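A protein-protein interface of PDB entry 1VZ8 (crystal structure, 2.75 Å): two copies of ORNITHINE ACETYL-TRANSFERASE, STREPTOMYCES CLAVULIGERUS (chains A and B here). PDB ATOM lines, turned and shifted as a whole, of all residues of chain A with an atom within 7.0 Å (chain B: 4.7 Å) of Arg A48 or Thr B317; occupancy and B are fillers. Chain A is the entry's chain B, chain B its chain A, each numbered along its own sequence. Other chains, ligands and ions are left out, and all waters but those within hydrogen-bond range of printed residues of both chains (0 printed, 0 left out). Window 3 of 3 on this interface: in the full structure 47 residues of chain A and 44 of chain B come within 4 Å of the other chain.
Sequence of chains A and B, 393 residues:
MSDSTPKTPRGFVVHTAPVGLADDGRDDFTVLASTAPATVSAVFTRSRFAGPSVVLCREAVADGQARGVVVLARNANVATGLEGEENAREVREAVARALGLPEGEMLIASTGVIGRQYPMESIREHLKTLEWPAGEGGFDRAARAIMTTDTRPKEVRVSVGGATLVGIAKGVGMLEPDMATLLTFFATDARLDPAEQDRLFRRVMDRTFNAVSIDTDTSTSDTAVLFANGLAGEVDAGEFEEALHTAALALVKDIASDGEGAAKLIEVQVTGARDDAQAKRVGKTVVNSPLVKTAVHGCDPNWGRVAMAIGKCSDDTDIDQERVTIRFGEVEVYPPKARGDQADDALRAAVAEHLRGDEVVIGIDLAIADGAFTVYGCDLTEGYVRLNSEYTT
The backbone carbonyl oxygen (O) of Gly B311 is in hydrogen-bond range of the backbone NH (N) of Arg A48 (2.9 Å).
The guanidinium group (NH1) of Arg A48 lies within hydrogen-bond range of the backbone carbonyl oxygen (O) of Thr B317, 3.0 Å away.
O of Ile B319 lies within hydrogen-bond range of NH1 of Arg A48.
NE2 of Gln B321 sits close to O of Arg A48, 3.4 Å away.
The side-chain amide nitrogen (NE2) of Gln B321 lies within hydrogen-bond range of the backbone carbonyl oxygen (O) of Ala A50 (3.2 Å).
The backbone carbonyl oxygen of Ile B310 sits close to the side-chain sulfur of Cys B313, 3.7 Å away.
OG1 of Thr A45 is in hydrogen-bond range of N of Ser A47 (3.0 Å).
OG of Ser A47 sits close to N of Phe A49, 3.1 Å away.
O of Arg A46 touches CB of Ser B314, at 3.5 Å.
Gly B311 touches Ser A47.
Cys B313 touches Arg A48 (O to CG, 3.2 Å).
O of Asp B316 touches CD of Arg A48, 2.9 Å away.
Phe A49 touches Gly B311 (CD1 to N, 3.9 Å).
Gln B321 touches Phe A49.
Of the printed residues of chain B, Arg A46 touches Ser B314 (3.5 Å).
Arg A48 touches just these residues of chain B: Gly B311 (2.9 Å), Cys B313 (3.2 Å), Asp B316 (2.9 Å), Thr B317 (3.0 Å), Ile B319 (2.6 Å) and Gln B321 (3.4 Å).
Thr B317 touches one residue of chain A.
Of the printed residues of chain A, Gln B321 touches Arg A48 (3.4 Å), Phe A49 (3.5 Å) and Ala A50 (3.2 Å).
The nearest residue of chain B that does not touch Arg A48 is Ser B314 (4.1 Å).
Hydrophobic or aromatic side chains of chain A within 4 Å of the printed part of chain B: Phe A49.
Along chain A the printed residues that touch a printed residue of chain B span positions 46 to 50.
Among the printed residues, 11 pairs touch across the chains.
No position is printed for both chains.
Of the 11 pairs that touch across the chains among the printed residues, none has its exchanged pair printed and touching as well.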
ATOM      1  N   THR A  45       0.789 -27.587 -10.208  1.00  0.00           N
ATOM      2  CA  THR A  45       1.889 -27.641  -9.264  1.00  0.00           C
ATOM      3  C   THR A  45       2.884 -26.515  -9.511  1.00  0.00           C
ATOM      4  O   THR A  45       2.918 -25.913 -10.584  1.00  0.00           O
ATOM      5  CB  THR A  45       2.662 -28.929  -9.385  1.00  0.00           C
ATOM      6  OG1 THR A  45       3.788 -28.868  -8.509  1.00  0.00           O
ATOM      7  CG2 THR A  45       3.126 -29.127 -10.824  1.00  0.00           C
ATOM      8  N   ARG A  46       3.711 -26.256  -8.510  1.00  0.00           N
ATOM      9  CA  ARG A  46       4.706 -25.194  -8.603  1.00  0.00           C
ATOM     10  C   ARG A  46       6.102 -25.766  -8.406  1.00  0.00           C
ATOM     11  O   ARG A  46       7.090 -25.050  -8.298  1.00  0.00           O
ATOM     12  CB  ARG A  46       4.401 -24.109  -7.563  1.00  0.00           C
ATOM     13  CG  ARG A  46       3.290 -23.168  -7.994  1.00  0.00           C
ATOM     14  CD  ARG A  46       2.978 -22.106  -6.938  1.00  0.00           C
ATOM     15  NE  ARG A  46       1.972 -22.558  -5.973  1.00  0.00           N
ATOM     16  CZ  ARG A  46       1.344 -21.763  -5.106  1.00  0.00           C
ATOM     17  NH1 ARG A  46       1.616 -20.462  -5.059  1.00  0.00           N
ATOM     18  NH2 ARG A  46       0.413 -22.264  -4.307  1.00  0.00           N
ATOM     19  N   SER A  47       6.158 -27.083  -8.370  1.00  0.00           N
ATOM     20  CA  SER A  47       7.399 -27.801  -8.201  1.00  0.00           C
ATOM     21  C   SER A  47       8.520 -27.198  -9.038  1.00  0.00           C
ATOM     22  O   SER A  47       8.313 -26.794 -10.187  1.00  0.00           O
ATOM     23  CB  SER A  47       7.187 -29.254  -8.601  1.00  0.00           C
ATOM     24  OG  SER A  47       8.340 -30.003  -8.318  1.00  0.00           O
ATOM     25  N   ARG A  48       9.708 -27.128  -8.453  1.00  0.00           N
ATOM     26  CA  ARG A  48      10.864 -26.606  -9.164  1.00  0.00           C
ATOM     27  C   ARG A  48      11.213 -27.643 -10.224  1.00  0.00           C
ATOM     28  O   ARG A  48      11.933 -27.353 -11.169  1.00  0.00           O
ATOM     29  CB  ARG A  48      12.037 -26.430  -8.209  1.00  0.00           C
ATOM     30  CG  ARG A  48      11.776 -25.460  -7.079  1.00  0.00           C
ATOM     31  CD  ARG A  48      12.101 -24.039  -7.501  1.00  0.00           C
ATOM     32  NE  ARG A  48      11.177 -23.544  -8.514  1.00  0.00           N
ATOM     33  CZ  ARG A  48      11.558 -22.937  -9.634  1.00  0.00           C
ATOM     34  NH1 ARG A  48      12.848 -22.752  -9.883  1.00  0.00           N
ATOM     35  NH2 ARG A  48      10.647 -22.521 -10.503  1.00  0.00           N
ATOM     36  N   PHE A  49      10.699 -28.857 -10.041  1.00  0.00           N
ATOM     37  CA  PHE A  49      10.915 -29.952 -10.973  1.00  0.00           C
ATOM     38  C   PHE A  49       9.652 -30.249 -11.773  1.00  0.00           C
ATOM     39  O   PHE A  49       9.339 -31.406 -12.031  1.00  0.00           O
ATOM     40  CB  PHE A  49      11.342 -31.218 -10.225  1.00  0.00           C
ATOM     41  CG  PHE A  49      12.832 -31.374 -10.113  1.00  0.00           C
ATOM     42  CD1 PHE A  49      13.539 -30.786  -9.061  1.00  0.00           C
ATOM     43  CD2 PHE A  49      13.544 -32.059 -11.092  1.00  0.00           C
ATOM     44  CE1 PHE A  49      14.944 -30.878  -8.993  1.00  0.00           C
ATOM     45  CE2 PHE A  49      14.936 -32.155 -11.033  1.00  0.00           C
ATOM     46  CZ  PHE A  49      15.636 -31.560  -9.978  1.00  0.00           C
ATOM     47  N   ALA A  50       8.921 -29.219 -12.177  1.00  0.00           N
ATOM     48  CA  ALA A  50       7.681 -29.456 -12.916  1.00  0.00           C
ATOM     49  C   ALA A  50       7.939 -29.903 -14.343  1.00  0.00           C
ATOM     50  O   ALA A  50       8.645 -29.233 -15.095  1.00  0.00           O
ATOM     51  CB  ALA A  50       6.806 -28.203 -12.901  1.00  0.00           C
ATOM     52  N   GLY A  51       7.353 -31.037 -14.706  1.00  0.00           N
ATOM     53  CA  GLY A  51       7.528 -31.585 -16.039  1.00  0.00           C
ATOM     54  C   GLY A  51       7.064 -30.711 -17.185  1.00  0.00           C
ATOM     55  O   GLY A  51       6.244 -29.817 -16.993  1.00  0.00           O
ATOM     56  N   SER A 219       3.839 -33.286  -5.727  1.00  0.00           N
ATOM     57  CA  SER A 219       4.241 -33.771  -7.036  1.00  0.00           C
ATOM     58  C   SER A 219       4.720 -32.744  -8.046  1.00  0.00           C
ATOM     59  O   SER A 219       4.466 -31.552  -7.915  1.00  0.00           O
ATOM     60  CB  SER A 219       3.084 -34.539  -7.660  1.00  0.00           C
ATOM     61  OG  SER A 219       3.319 -34.733  -9.043  1.00  0.00           O
ATOM     62  N   THR A 220       5.391 -33.253  -9.077  1.00  0.00           N
ATOM     63  CA  THR A 220       5.942 -32.459 -10.169  1.00  0.00           C
ATOM     64  C   THR A 220       4.943 -32.403 -11.326  1.00  0.00           C
ATOM     65  O   THR A 220       5.250 -31.901 -12.402  1.00  0.00           O
ATOM     66  CB  THR A 220       7.170 -33.136 -10.723  1.00  0.00           C
ATOM     67  OG1 THR A 220       6.814 -34.472 -11.109  1.00  0.00           O
ATOM     68  CG2 THR A 220       8.269 -33.185  -9.693  1.00  0.00           C
ATOM     69  N   ILE B 310      13.171 -32.087  -3.750  1.00  0.00           N
ATOM     70  CA  ILE B 310      13.763 -30.779  -3.940  1.00  0.00           C
ATOM     71  C   ILE B 310      12.784 -29.781  -4.549  1.00  0.00           C
ATOM     72  O   ILE B 310      12.731 -28.636  -4.114  1.00  0.00           O
ATOM     73  CB  ILE B 310      15.009 -30.862  -4.807  1.00  0.00           C
ATOM     74  CG1 ILE B 310      16.139 -31.526  -4.024  1.00  0.00           C
ATOM     75  CG2 ILE B 310      15.442 -29.461  -5.225  1.00  0.00           C
ATOM     76  CD1 ILE B 310      17.381 -31.772  -4.848  1.00  0.00           C
ATOM     77  N   GLY B 311      12.003 -30.206  -5.540  1.00  0.00           N
ATOM     78  CA  GLY B 311      11.065 -29.292  -6.173  1.00  0.00           C
ATOM     79  C   GLY B 311       9.979 -28.735  -5.263  1.00  0.00           C
ATOM     80  O   GLY B 311       9.242 -27.824  -5.638  1.00  0.00           O
ATOM     81  N   CYS B 313      10.527 -27.185  -2.605  1.00  0.00           N
ATOM     82  CA  CYS B 313      10.945 -25.860  -2.165  1.00  0.00           C
ATOM     83  C   CYS B 313      10.565 -24.965  -3.347  1.00  0.00           C
ATOM     84  O   CYS B 313      11.420 -24.409  -4.035  1.00  0.00           O
ATOM     85  CB  CYS B 313      12.457 -25.830  -1.898  1.00  0.00           C
ATOM     86  SG  CYS B 313      13.018 -27.095  -0.716  1.00  0.00           S
ATOM     87  N   SER B 314       9.255 -24.852  -3.569  1.00  0.00           N
ATOM     88  CA  SER B 314       8.690 -24.085  -4.672  1.00  0.00           C
ATOM     89  C   SER B 314       8.881 -22.579  -4.661  1.00  0.00           C
ATOM     90  O   SER B 314       8.716 -21.947  -5.699  1.00  0.00           O
ATOM     91  CB  SER B 314       7.205 -24.409  -4.819  1.00  0.00           C
ATOM     92  OG  SER B 314       6.558 -24.431  -3.564  1.00  0.00           O
ATOM     93  N   ASP B 315       9.224 -21.998  -3.516  1.00  0.00           N
ATOM     94  CA  ASP B 315       9.451 -20.554  -3.463  1.00  0.00           C
ATOM     95  C   ASP B 315      10.910 -20.253  -3.793  1.00  0.00           C
ATOM     96  O   ASP B 315      11.307 -19.098  -3.979  1.00  0.00           O
ATOM     97  CB  ASP B 315       9.121 -19.981  -2.084  1.00  0.00           C
ATOM     98  CG  ASP B 315       7.629 -19.921  -1.812  1.00  0.00           C
ATOM     99  OD1 ASP B 315       6.828 -19.856  -2.786  1.00  0.00           O
ATOM    100  OD2 ASP B 315       7.270 -19.922  -0.613  1.00  0.00           O
ATOM    101  N   ASP B 316      11.707 -21.309  -3.862  1.00  0.00           N
ATOM    102  CA  ASP B 316      13.105 -21.153  -4.177  1.00  0.00           C
ATOM    103  C   ASP B 316      13.290 -21.175  -5.680  1.00  0.00           C
ATOM    104  O   ASP B 316      13.906 -22.081  -6.246  1.00  0.00           O
ATOM    105  CB  ASP B 316      13.900 -22.256  -3.500  1.00  0.00           C
ATOM    106  CG  ASP B 316      13.923 -22.096  -2.009  1.00  0.00           C
ATOM    107  OD1 ASP B 316      13.033 -22.639  -1.322  1.00  0.00           O
ATOM    108  OD2 ASP B 316      14.828 -21.395  -1.530  1.00  0.00           O
ATOM    109  N   THR B 317      12.742 -20.149  -6.316  1.00  0.00           N
ATOM    110  CA  THR B 317      12.796 -19.991  -7.762  1.00  0.00           C
ATOM    111  C   THR B 317      14.205 -20.028  -8.379  1.00  0.00           C
ATOM    112  O   THR B 317      14.348 -20.159  -9.591  1.00  0.00           O
ATOM    113  CB  THR B 317      12.127 -18.677  -8.166  1.00  0.00           C
ATOM    114  OG1 THR B 317      12.903 -17.578  -7.668  1.00  0.00           O
ATOM    115  CG2 THR B 317      10.720 -18.605  -7.604  1.00  0.00           C
ATOM    116  N   ASP B 318      15.246 -19.912  -7.564  1.00  0.00           N
ATOM    117  CA  ASP B 318      16.593 -19.936  -8.115  1.00  0.00           C
ATOM    118  C   ASP B 318      17.115 -21.369  -8.235  1.00  0.00           C
ATOM    119  O   ASP B 318      18.179 -21.610  -8.810  1.00  0.00           O
ATOM    120  CB  ASP B 318      17.528 -19.048  -7.282  1.00  0.00           C
ATOM    121  CG  ASP B 318      17.698 -19.543  -5.855  1.00  0.00           C
ATOM    122  OD1 ASP B 318      16.723 -20.114  -5.306  1.00  0.00           O
ATOM    123  OD2 ASP B 318      18.800 -19.338  -5.279  1.00  0.00           O
ATOM    124  N   ILE B 319      16.365 -22.320  -7.687  1.00  0.00           N
ATOM    125  CA  ILE B 319      16.738 -23.722  -7.810  1.00  0.00           C
ATOM    126  C   ILE B 319      16.298 -24.104  -9.216  1.00  0.00           C
ATOM    127  O   ILE B 319      15.117 -24.014  -9.553  1.00  0.00           O
ATOM    128  CB  ILE B 319      16.007 -24.609  -6.796  1.00  0.00           C
ATOM    129  CG1 ILE B 319      16.522 -24.309  -5.399  1.00  0.00           C
ATOM    130  CG2 ILE B 319      16.245 -26.064  -7.112  1.00  0.00           C
ATOM    131  CD1 ILE B 319      16.103 -25.326  -4.373  1.00  0.00           C
ATOM    132  N   GLN B 321      15.717 -26.788 -12.210  1.00  0.00           N
ATOM    133  CA  GLN B 321      15.498 -28.171 -12.556  1.00  0.00           C
ATOM    134  C   GLN B 321      16.690 -28.795 -13.256  1.00  0.00           C
ATOM    135  O   GLN B 321      17.020 -29.949 -13.013  1.00  0.00           O
ATOM    136  CB  GLN B 321      14.274 -28.264 -13.452  1.00  0.00           C
ATOM    137  CG  GLN B 321      13.957 -29.666 -13.905  1.00  0.00           C
ATOM    138  CD  GLN B 321      12.481 -29.880 -14.147  1.00  0.00           C
ATOM    139  OE1 GLN B 321      12.033 -31.015 -14.252  1.00  0.00           O
ATOM    140  NE2 GLN B 321      11.717 -28.796 -14.237  1.00  0.00           N
